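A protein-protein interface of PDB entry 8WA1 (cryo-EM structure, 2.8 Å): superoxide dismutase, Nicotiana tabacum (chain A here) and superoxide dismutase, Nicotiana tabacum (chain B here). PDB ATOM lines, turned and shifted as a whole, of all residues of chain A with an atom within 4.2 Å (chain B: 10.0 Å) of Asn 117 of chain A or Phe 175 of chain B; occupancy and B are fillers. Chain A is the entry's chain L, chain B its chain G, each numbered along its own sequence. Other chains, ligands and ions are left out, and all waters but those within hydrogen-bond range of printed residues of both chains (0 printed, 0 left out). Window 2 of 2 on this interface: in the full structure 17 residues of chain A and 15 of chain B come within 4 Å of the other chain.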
ATOM      1  N   PRO A 114     -25.379  -9.722  31.769  1.00  0.00           N
ATOM      2  CA  PRO A 114     -25.127  -9.897  30.337  1.00  0.00           C
ATOM      3  C   PRO A 114     -26.314 -10.396  29.508  1.00  0.00           C
ATOM      4  O   PRO A 114     -26.487  -9.925  28.391  1.00  0.00           O
ATOM      5  CB  PRO A 114     -23.976 -10.901  30.307  1.00  0.00           C
ATOM      6  CG  PRO A 114     -23.257 -10.678  31.593  1.00  0.00           C
ATOM      7  CD  PRO A 114     -24.300 -10.283  32.601  1.00  0.00           C
ATOM      8  N   PRO A 115     -27.213 -11.265  30.047  1.00  0.00           N
ATOM      9  CA  PRO A 115     -28.324 -11.571  29.137  1.00  0.00           C
ATOM     10  C   PRO A 115     -29.405 -10.501  29.075  1.00  0.00           C
ATOM     11  O   PRO A 115     -30.527 -10.843  28.730  1.00  0.00           O
ATOM     12  CB  PRO A 115     -28.900 -12.867  29.695  1.00  0.00           C
ATOM     13  CG  PRO A 115     -27.810 -13.455  30.507  1.00  0.00           C
ATOM     14  CD  PRO A 115     -27.249 -12.244  31.166  1.00  0.00           C
ATOM     15  N   PHE A 116     -29.108  -9.245  29.379  1.00  0.00           N
ATOM     16  CA  PHE A 116     -30.144  -8.223  29.231  1.00  0.00           C
ATOM     17  C   PHE A 116     -30.109  -7.535  27.900  1.00  0.00           C
ATOM     18  O   PHE A 116     -31.079  -7.578  27.154  1.00  0.00           O
ATOM     19  CB  PHE A 116     -30.073  -7.156  30.313  1.00  0.00           C
ATOM     20  CG  PHE A 116     -31.147  -6.116  30.193  1.00  0.00           C
ATOM     21  CD1 PHE A 116     -32.479  -6.475  30.198  1.00  0.00           C
ATOM     22  CD2 PHE A 116     -30.823  -4.785  30.048  1.00  0.00           C
ATOM     23  CE1 PHE A 116     -33.464  -5.520  30.073  1.00  0.00           C
ATOM     24  CE2 PHE A 116     -31.803  -3.824  29.929  1.00  0.00           C
ATOM     25  CZ  PHE A 116     -33.129  -4.191  29.940  1.00  0.00           C
ATOM     26  N   ASN A 117     -29.005  -6.872  27.614  1.00  0.00           N
ATOM     27  CA  ASN A 117     -28.933  -6.106  26.388  1.00  0.00           C
ATOM     28  C   ASN A 117     -29.363  -6.880  25.150  1.00  0.00           C
ATOM     29  O   ASN A 117     -30.058  -6.322  24.310  1.00  0.00           O
ATOM     30  CB  ASN A 117     -27.548  -5.462  26.203  1.00  0.00           C
ATOM     31  CG  ASN A 117     -26.451  -6.476  25.942  1.00  0.00           C
ATOM     32  OD1 ASN A 117     -26.362  -7.504  26.610  1.00  0.00           O
ATOM     33  ND2 ASN A 117     -25.607  -6.187  24.962  1.00  0.00           N
ATOM     34  N   ASN A 118     -29.004  -8.157  25.036  1.00  0.00           N
ATOM     35  CA  ASN A 118     -29.328  -8.855  23.801  1.00  0.00           C
ATOM     36  C   ASN A 118     -30.806  -9.134  23.744  1.00  0.00           C
ATOM     37  O   ASN A 118     -31.447  -8.930  22.713  1.00  0.00           O
ATOM     38  CB  ASN A 118     -28.541 -10.152  23.703  1.00  0.00           C
ATOM     39  CG  ASN A 118     -27.061  -9.912  23.518  1.00  0.00           C
ATOM     40  OD1 ASN A 118     -26.642  -8.806  23.180  1.00  0.00           O
ATOM     41  ND2 ASN A 118     -26.260 -10.943  23.735  1.00  0.00           N
ATOM     42  N   ALA A 119     -31.360  -9.577  24.862  1.00  0.00           N
ATOM     43  CA  ALA A 119     -32.764  -9.938  24.879  1.00  0.00           C
ATOM     44  C   ALA A 119     -33.640  -8.758  24.574  1.00  0.00           C
ATOM     45  O   ALA A 119     -34.557  -8.851  23.764  1.00  0.00           O
ATOM     46  CB  ALA A 119     -33.131 -10.492  26.241  1.00  0.00           C
ATOM     47  N   ALA A 120     -33.342  -7.631  25.192  1.00  0.00           N
ATOM     48  CA  ALA A 120     -34.187  -6.476  25.009  1.00  0.00           C
ATOM     49  C   ALA A 120     -34.147  -6.050  23.578  1.00  0.00           C
ATOM     50  O   ALA A 120     -35.161  -5.692  23.016  1.00  0.00           O
ATOM     51  CB  ALA A 120     -33.736  -5.347  25.903  1.00  0.00           C
ATOM     52  N   GLN A 121     -32.971  -6.089  22.980  1.00  0.00           N
ATOM     53  CA  GLN A 121     -32.851  -5.612  21.623  1.00  0.00           C
ATOM     54  C   GLN A 121     -33.678  -6.433  20.668  1.00  0.00           C
ATOM     55  O   GLN A 121     -34.351  -5.884  19.812  1.00  0.00           O
ATOM     56  CB  GLN A 121     -31.397  -5.639  21.196  1.00  0.00           C
ATOM     57  CG  GLN A 121     -30.617  -4.428  21.650  1.00  0.00           C
ATOM     58  CD  GLN A 121     -31.017  -3.181  20.898  1.00  0.00           C
ATOM     59  OE1 GLN A 121     -31.274  -3.221  19.696  1.00  0.00           O
ATOM     60  NE2 GLN A 121     -31.060  -2.060  21.601  1.00  0.00           N
ATOM     61  N   ASN A 208     -29.767   3.051  24.858  1.00  0.00           N
ATOM     62  CA  ASN A 208     -29.477   1.793  24.179  1.00  0.00           C
ATOM     63  C   ASN A 208     -29.848   0.595  25.046  1.00  0.00           C
ATOM     64  O   ASN A 208     -29.530   0.546  26.238  1.00  0.00           O
ATOM     65  CB  ASN A 208     -27.995   1.729  23.795  1.00  0.00           C
ATOM     66  CG  ASN A 208     -27.082   2.198  24.911  1.00  0.00           C
ATOM     67  OD1 ASN A 208     -27.541   2.552  25.996  1.00  0.00           O
ATOM     68  ND2 ASN A 208     -25.780   2.201  24.649  1.00  0.00           N
ATOM     69  N   ALA A 209     -30.568  -0.352  24.435  1.00  0.00           N
ATOM     70  CA  ALA A 209     -30.968  -1.619  25.044  1.00  0.00           C
ATOM     71  C   ALA A 209     -31.990  -1.430  26.160  1.00  0.00           C
ATOM     72  O   ALA A 209     -32.391  -2.403  26.807  1.00  0.00           O
ATOM     73  CB  ALA A 209     -29.751  -2.388  25.567  1.00  0.00           C
ATOM     74  N   TRP A 226     -31.874   4.098  15.684  1.00  0.00           N
ATOM     75  CA  TRP A 226     -30.516   3.622  15.740  1.00  0.00           C
ATOM     76  C   TRP A 226     -30.092   3.849  14.331  1.00  0.00           C
ATOM     77  O   TRP A 226     -30.921   3.897  13.431  1.00  0.00           O
ATOM     78  CB  TRP A 226     -30.447   2.138  16.045  1.00  0.00           C
ATOM     79  CG  TRP A 226     -30.407   1.774  17.494  1.00  0.00           C
ATOM     80  CD1 TRP A 226     -31.335   2.072  18.438  1.00  0.00           C
ATOM     81  CD2 TRP A 226     -29.398   1.006  18.156  1.00  0.00           C
ATOM     82  NE1 TRP A 226     -30.965   1.557  19.652  1.00  0.00           N
ATOM     83  CE2 TRP A 226     -29.776   0.894  19.505  1.00  0.00           C
ATOM     84  CE3 TRP A 226     -28.206   0.411  17.740  1.00  0.00           C
ATOM     85  CZ2 TRP A 226     -29.008   0.214  20.440  1.00  0.00           C
ATOM     86  CZ3 TRP A 226     -27.445  -0.267  18.670  1.00  0.00           C
ATOM     87  CH2 TRP A 226     -27.849  -0.360  20.006  1.00  0.00           C
ATOM     88  N   GLU B 169     -10.687  -6.367  22.215  1.00  0.00           N
ATOM     89  CA  GLU B 169     -11.709  -6.872  23.124  1.00  0.00           C
ATOM     90  C   GLU B 169     -12.579  -5.741  23.659  1.00  0.00           C
ATOM     91  O   GLU B 169     -13.807  -5.859  23.709  1.00  0.00           O
ATOM     92  CB  GLU B 169     -11.048  -7.645  24.269  1.00  0.00           C
ATOM     93  CG  GLU B 169     -12.017  -8.186  25.313  1.00  0.00           C
ATOM     94  CD  GLU B 169     -12.218  -7.232  26.476  1.00  0.00           C
ATOM     95  OE1 GLU B 169     -11.505  -6.209  26.540  1.00  0.00           O
ATOM     96  OE2 GLU B 169     -13.088  -7.507  27.330  1.00  0.00           O
ATOM     97  N   ALA B 170     -11.956  -4.630  24.063  1.00  0.00           N
ATOM     98  CA  ALA B 170     -12.723  -3.495  24.564  1.00  0.00           C
ATOM     99  C   ALA B 170     -13.545  -2.840  23.464  1.00  0.00           C
ATOM    100  O   ALA B 170     -14.655  -2.361  23.724  1.00  0.00           O
ATOM    101  CB  ALA B 170     -11.788  -2.473  25.211  1.00  0.00           C
ATOM    102  N   ALA B 171     -13.022  -2.800  22.236  1.00  0.00           N
ATOM    103  CA  ALA B 171     -13.771  -2.199  21.137  1.00  0.00           C
ATOM    104  C   ALA B 171     -14.993  -3.036  20.779  1.00  0.00           C
ATOM    105  O   ALA B 171     -16.068  -2.492  20.499  1.00  0.00           O
ATOM    106  CB  ALA B 171     -12.862  -2.020  19.921  1.00  0.00           C
ATOM    107  N   LEU B 172     -14.849  -4.363  20.781  1.00  0.00           N
ATOM    108  CA  LEU B 172     -15.982  -5.226  20.459  1.00  0.00           C
ATOM    109  C   LEU B 172     -16.967  -5.306  21.620  1.00  0.00           C
ATOM    110  O   LEU B 172     -18.173  -5.486  21.409  1.00  0.00           O
ATOM    111  CB  LEU B 172     -15.489  -6.623  20.074  1.00  0.00           C
ATOM    112  CG  LEU B 172     -15.180  -6.889  18.596  1.00  0.00           C
ATOM    113  CD1 LEU B 172     -14.062  -5.995  18.080  1.00  0.00           C
ATOM    114  CD2 LEU B 172     -14.836  -8.355  18.385  1.00  0.00           C
ATOM    115  N   ALA B 173     -16.473  -5.181  22.854  1.00  0.00           N
ATOM    116  CA  ALA B 173     -17.336  -5.345  24.020  1.00  0.00           C
ATOM    117  C   ALA B 173     -18.314  -4.185  24.162  1.00  0.00           C
ATOM    118  O   ALA B 173     -19.460  -4.380  24.585  1.00  0.00           O
ATOM    119  CB  ALA B 173     -16.488  -5.489  25.283  1.00  0.00           C
ATOM    120  N   LEU B 174     -17.878  -2.971  23.828  1.00  0.00           N
ATOM    121  CA  LEU B 174     -18.736  -1.800  23.956  1.00  0.00           C
ATOM    122  C   LEU B 174     -19.971  -1.951  23.078  1.00  0.00           C
ATOM    123  O   LEU B 174     -19.869  -2.123  21.860  1.00  0.00           O
ATOM    124  CB  LEU B 174     -17.956  -0.536  23.577  1.00  0.00           C
ATOM    125  CG  LEU B 174     -18.385   0.789  24.216  1.00  0.00           C
ATOM    126  CD1 LEU B 174     -17.245   1.796  24.164  1.00  0.00           C
ATOM    127  CD2 LEU B 174     -19.631   1.365  23.553  1.00  0.00           C
ATOM    128  N   PHE B 175     -21.142  -1.888  23.707  1.00  0.00           N
ATOM    129  CA  PHE B 175     -22.412  -2.135  23.031  1.00  0.00           C
ATOM    130  C   PHE B 175     -23.107  -0.804  22.773  1.00  0.00           C
ATOM    131  O   PHE B 175     -23.533  -0.124  23.713  1.00  0.00           O
ATOM    132  CB  PHE B 175     -23.297  -3.060  23.859  1.00  0.00           C
ATOM    133  CG  PHE B 175     -24.661  -3.264  23.274  1.00  0.00           C
ATOM    134  CD1 PHE B 175     -24.844  -4.112  22.194  1.00  0.00           C
ATOM    135  CD2 PHE B 175     -25.761  -2.602  23.795  1.00  0.00           C
ATOM    136  CE1 PHE B 175     -26.098  -4.298  21.649  1.00  0.00           C
ATOM    137  CE2 PHE B 175     -27.015  -2.785  23.253  1.00  0.00           C
ATOM    138  CZ  PHE B 175     -27.182  -3.633  22.178  1.00  0.00           C
ATOM    139  N   GLY B 176     -23.219  -0.435  21.501  1.00  0.00           N
ATOM    140  CA  GLY B 176     -23.877   0.802  21.136  1.00  0.00           C
ATOM    141  C   GLY B 176     -22.927   1.777  20.476  1.00  0.00           C
ATOM    142  O   GLY B 176     -22.178   1.410  19.565  1.00  0.00           O
ATOM    143  N   SER B 177     -23.027   3.047  20.862  1.00  0.00           N
ATOM    144  CA  SER B 177     -22.192   4.085  20.265  1.00  0.00           C
ATOM    145  C   SER B 177     -21.273   4.662  21.318  1.00  0.00           C
ATOM    146  O   SER B 177     -21.668   4.809  22.469  1.00  0.00           O
ATOM    147  CB  SER B 177     -23.067   5.186  19.691  1.00  0.00           C
ATOM    148  OG  SER B 177     -23.794   4.721  18.571  1.00  0.00           O
ATOM    149  N   GLY B 178     -20.049   4.990  20.941  1.00  0.00           N
ATOM    150  CA  GLY B 178     -19.095   5.463  21.921  1.00  0.00           C
ATOM    151  C   GLY B 178     -17.725   5.598  21.314  1.00  0.00           C
ATOM    152  O   GLY B 178     -17.599   5.591  20.099  1.00  0.00           O
ATOM    153  N   TRP B 179     -16.703   5.777  22.140  1.00  0.00           N
ATOM    154  CA  TRP B 179     -15.344   5.859  21.645  1.00  0.00           C
ATOM    155  C   TRP B 179     -14.449   5.050  22.574  1.00  0.00           C
ATOM    156  O   TRP B 179     -14.826   4.801  23.713  1.00  0.00           O
ATOM    157  CB  TRP B 179     -14.887   7.310  21.603  1.00  0.00           C
ATOM    158  CG  TRP B 179     -15.657   8.222  20.688  1.00  0.00           C
ATOM    159  CD1 TRP B 179     -16.943   8.651  20.839  1.00  0.00           C
ATOM    160  CD2 TRP B 179     -15.167   8.852  19.505  1.00  0.00           C
ATOM    161  NE1 TRP B 179     -17.292   9.482  19.810  1.00  0.00           N
ATOM    162  CE2 TRP B 179     -16.216   9.626  18.979  1.00  0.00           C
ATOM    163  CE3 TRP B 179     -13.945   8.835  18.838  1.00  0.00           C
ATOM    164  CZ2 TRP B 179     -16.079  10.365  17.814  1.00  0.00           C
ATOM    165  CZ3 TRP B 179     -13.812   9.567  17.686  1.00  0.00           C
ATOM    166  CH2 TRP B 179     -14.870  10.324  17.185  1.00  0.00           C
ATOM    167  N   LYS B 195     -13.087   2.962  27.645  1.00  0.00           N
ATOM    168  CA  LYS B 195     -14.211   2.968  26.726  1.00  0.00           C
ATOM    169  C   LYS B 195     -15.239   3.917  27.266  1.00  0.00           C
ATOM    170  O   LYS B 195     -15.654   3.782  28.408  1.00  0.00           O
ATOM    171  CB  LYS B 195     -14.847   1.600  26.690  1.00  0.00           C
ATOM    172  CG  LYS B 195     -13.876   0.442  26.626  1.00  0.00           C
ATOM    173  CD  LYS B 195     -14.611  -0.853  26.921  1.00  0.00           C
ATOM    174  CE  LYS B 195     -15.349  -0.763  28.246  1.00  0.00           C
ATOM    175  NZ  LYS B 195     -16.115  -2.003  28.541  1.00  0.00           N
ATOM    176  N   THR B 196     -15.671   4.869  26.456  1.00  0.00           N
ATOM    177  CA  THR B 196     -16.613   5.867  26.925  1.00  0.00           C
ATOM    178  C   THR B 196     -17.872   5.839  26.101  1.00  0.00           C
ATOM    179  O   THR B 196     -17.803   5.856  24.892  1.00  0.00           O
ATOM    180  CB  THR B 196     -16.021   7.273  26.807  1.00  0.00           C
ATOM    181  OG1 THR B 196     -15.637   7.515  25.450  1.00  0.00           O
ATOM    182  CG2 THR B 196     -14.802   7.417  27.694  1.00  0.00           C
ATOM    183  N   SER B 197     -19.022   5.806  26.754  1.00  0.00           N
ATOM    184  CA  SER B 197     -20.292   5.808  26.045  1.00  0.00           C
ATOM    185  C   SER B 197     -20.611   7.124  25.379  1.00  0.00           C
ATOM    186  O   SER B 197     -20.369   8.174  25.959  1.00  0.00           O
ATOM    187  CB  SER B 197     -21.414   5.468  27.010  1.00  0.00           C
ATOM    188  OG  SER B 197     -22.668   5.844  26.475  1.00  0.00           O
ATOM    189  N   ASN B 198     -21.150   7.076  24.167  1.00  0.00           N
ATOM    190  CA  ASN B 198     -21.562   8.294  23.474  1.00  0.00           C
ATOM    191  C   ASN B 198     -20.479   9.336  23.289  1.00  0.00           C
ATOM    192  O   ASN B 198     -19.406   9.033  22.786  1.00  0.00           O
ATOM    193  CB  ASN B 198     -22.786   8.918  24.136  1.00  0.00           C
ATOM    194  CG  ASN B 198     -24.054   8.145  23.854  1.00  0.00           C
ATOM    195  OD1 ASN B 198     -24.023   7.097  23.211  1.00  0.00           O
ATOM    196  ND2 ASN B 198     -25.180   8.661  24.332  1.00  0.00           N
ATOM    197  N   LEU B 215     -16.751   4.598  17.606  1.00  0.00           N
ATOM    198  CA  LEU B 215     -17.556   3.392  17.585  1.00  0.00           C
ATOM    199  C   LEU B 215     -18.981   3.750  17.273  1.00  0.00           C
ATOM    200  O   LEU B 215     -19.857   2.898  17.314  1.00  0.00           O
ATOM    201  CB  LEU B 215     -17.468   2.633  18.899  1.00  0.00           C
ATOM    202  CG  LEU B 215     -16.095   2.037  19.188  1.00  0.00           C
ATOM    203  CD1 LEU B 215     -16.144   1.224  20.468  1.00  0.00           C
ATOM    204  CD2 LEU B 215     -15.651   1.167  18.023  1.00  0.00           C
ATOM    205  N   TRP B 216     -19.239   5.016  16.989  1.00  0.00           N
ATOM    206  CA  TRP B 216     -20.574   5.368  16.564  1.00  0.00           C
ATOM    207  C   TRP B 216     -20.745   4.711  15.209  1.00  0.00           C
ATOM    208  O   TRP B 216     -19.814   4.680  14.413  1.00  0.00           O
ATOM    209  CB  TRP B 216     -20.765   6.876  16.486  1.00  0.00           C
ATOM    210  CG  TRP B 216     -20.938   7.546  17.806  1.00  0.00           C
ATOM    211  CD1 TRP B 216     -20.103   7.473  18.876  1.00  0.00           C
ATOM    212  CD2 TRP B 216     -22.008   8.413  18.192  1.00  0.00           C
ATOM    213  NE1 TRP B 216     -20.590   8.228  19.911  1.00  0.00           N
ATOM    214  CE2 TRP B 216     -21.760   8.819  19.515  1.00  0.00           C
ATOM    215  CE3 TRP B 216     -23.157   8.879  17.550  1.00  0.00           C
ATOM    216  CZ2 TRP B 216     -22.615   9.671  20.207  1.00  0.00           C
ATOM    217  CZ3 TRP B 216     -24.004   9.727  18.238  1.00  0.00           C
ATOM    218  CH2 TRP B 216     -23.728  10.114  19.553  1.00  0.00           C
ATOM    219  N   GLU B 217     -21.934   4.208  14.922  1.00  0.00           N
ATOM    220  CA  GLU B 217     -22.159   3.473  13.681  1.00  0.00           C
ATOM    221  C   GLU B 217     -21.974   4.288  12.436  1.00  0.00           C
ATOM    222  O   GLU B 217     -21.598   3.748  11.403  1.00  0.00           O
ATOM    223  CB  GLU B 217     -23.536   2.821  13.679  1.00  0.00           C
ATOM    224  CG  GLU B 217     -23.808   1.966  14.905  1.00  0.00           C
ATOM    225  CD  GLU B 217     -25.164   1.296  14.861  1.00  0.00           C
ATOM    226  OE1 GLU B 217     -25.911   1.520  13.888  1.00  0.00           O
ATOM    227  OE2 GLU B 217     -25.482   0.542  15.802  1.00  0.00           O
ATOM    228  N   TYR B 220     -18.819   3.553  10.529  1.00  0.00           N
ATOM    229  CA  TYR B 220     -18.548   2.330   9.770  1.00  0.00           C
ATOM    230  C   TYR B 220     -19.628   1.685   8.918  1.00  0.00           C
ATOM    231  O   TYR B 220     -19.299   0.877   8.061  1.00  0.00           O
ATOM    232  CB  TYR B 220     -17.967   1.264  10.704  1.00  0.00           C
ATOM    233  CG  TYR B 220     -18.880   0.841  11.829  1.00  0.00           C
ATOM    234  CD1 TYR B 220     -19.840  -0.141  11.639  1.00  0.00           C
ATOM    235  CD2 TYR B 220     -18.766   1.408  13.087  1.00  0.00           C
ATOM    236  CE1 TYR B 220     -20.673  -0.533  12.663  1.00  0.00           C
ATOM    237  CE2 TYR B 220     -19.593   1.018  14.120  1.00  0.00           C
ATOM    238  CZ  TYR B 220     -20.544   0.050  13.900  1.00  0.00           C
ATOM    239  OH  TYR B 220     -21.372  -0.342  14.923  1.00  0.00           O
ATOM    240  N   ASN B 226     -22.083  -4.472   9.303  1.00  0.00           N
ATOM    241  CA  ASN B 226     -22.258  -5.039  10.642  1.00  0.00           C
ATOM    242  C   ASN B 226     -21.075  -5.812  11.211  1.00  0.00           C
ATOM    243  O   ASN B 226     -21.225  -6.497  12.219  1.00  0.00           O
ATOM    244  CB  ASN B 226     -23.525  -5.896  10.698  1.00  0.00           C
ATOM    245  CG  ASN B 226     -24.786  -5.069  10.884  1.00  0.00           C
ATOM    246  OD1 ASN B 226     -25.770  -5.244  10.167  1.00  0.00           O
ATOM    247  ND2 ASN B 226     -24.751  -4.148  11.836  1.00  0.00           N
ATOM    248  N   LYS B 228     -18.055  -5.169  13.114  1.00  0.00           N
ATOM    249  CA  LYS B 228     -17.232  -4.246  13.888  1.00  0.00           C
ATOM    250  C   LYS B 228     -15.833  -4.802  14.111  1.00  0.00           C
ATOM    251  O   LYS B 228     -14.867  -4.034  14.199  1.00  0.00           O
ATOM    252  CB  LYS B 228     -17.904  -3.939  15.226  1.00  0.00           C
ATOM    253  CG  LYS B 228     -19.215  -3.176  15.104  1.00  0.00           C
ATOM    254  CD  LYS B 228     -19.905  -3.035  16.455  1.00  0.00           C
ATOM    255  CE  LYS B 228     -19.002  -2.361  17.477  1.00  0.00           C
ATOM    256  NZ  LYS B 228     -18.585  -1.000  17.046  1.00  0.00           N
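O of Phe 175 of chain B sits at hydrogen-bond distance from ND2 of Asn 208 of chain A, 3.4 Å away.
The side-chain amide oxygen (OD1) of Asn 117 of chain A lies close to the backbone carbonyl oxygen (O) of Pro 114 of chain A (3.0 Å).
ND2 of Asn 117 of chain A lies within hydrogen-bond range of OD1 of Asn 118 of chain A.
The side-chain amide nitrogen (NE2) of Gln 121 of chain A sits close to the backbone NH (N) of Ala 209 of chain A, at 3.3 Å.
Phe 175 of chain B touches Asn 117 of chain A.
CZ of Phe 175 of chain B touches CG of Gln 121 of chain A (3.6 Å).
Phe 175 of chain B touches Ala 209 of chain A (CE2 to CB, 3.6 Å).
Trp 226 of chain A touches Phe 175 of chain B (CH2 to CZ, 3.98 Å).
Trp 226 of chain A touches Glu 217 of chain B (CE3 to OE2, 3.3 Å).
Asn 117 of chain A touches just one residue of chain B: Phe 175 (3.5 Å).
Ala 119 of chain A touches none of the printed residues of chain B.
No residue of chain B comes within 4 Å of Ala 120 of chain A.
Printed residues of chain B within 4 Å of Trp 226 of chain A: Phe 175 (3.98 Å) and Glu 217 (3.3 Å).
Printed residues of chain A within 4 Å of Glu 217 of chain B: Trp 226.
Printed residues of chain B within 4 Å of Asn 208 of chain A: Phe 175.
Of the printed residues of chain B, Gln 121 of chain A touches Phe 175.
Thr 196 of chain B touches none of the printed residues of chain A.
Trp 179 of chain B touches none of the printed residues of chain A.
The nearest residue of chain B that does not touch Asn 117 of chain A is Ala 173 of chain B (6.4 Å).
The nearest printed residue of chain A that does not touch Phe 175 of chain B is Asn 118 of chain A (4.8 Å).
The nearest printed residue of chain B that does not touch Trp 226 of chain A is Gly 176 of chain B (4.3 Å).
Printed residues of chain A that touch a printed residue of chain B: Asn 117, Gln 121, Asn 208, Ala 209 and Trp 226.
Hydrophobic or aromatic side chains of chain A within 4 Å of the printed part of chain B: Ala 209 and Trp 226.
Of the 21 printed residues of chain B, 2 touch a printed residue of chain A.
Printed residues of chain B that touch a printed residue of chain A: Phe 175 and Glu 217.
Hydrophobic or aromatic side chains of chain B that line the printed part of chain A: Phe 175.
Among the printed residues, no Asp or Glu carboxylate lies within 4 Å of a Lys or Arg side-chain nitrogen of the other chain.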
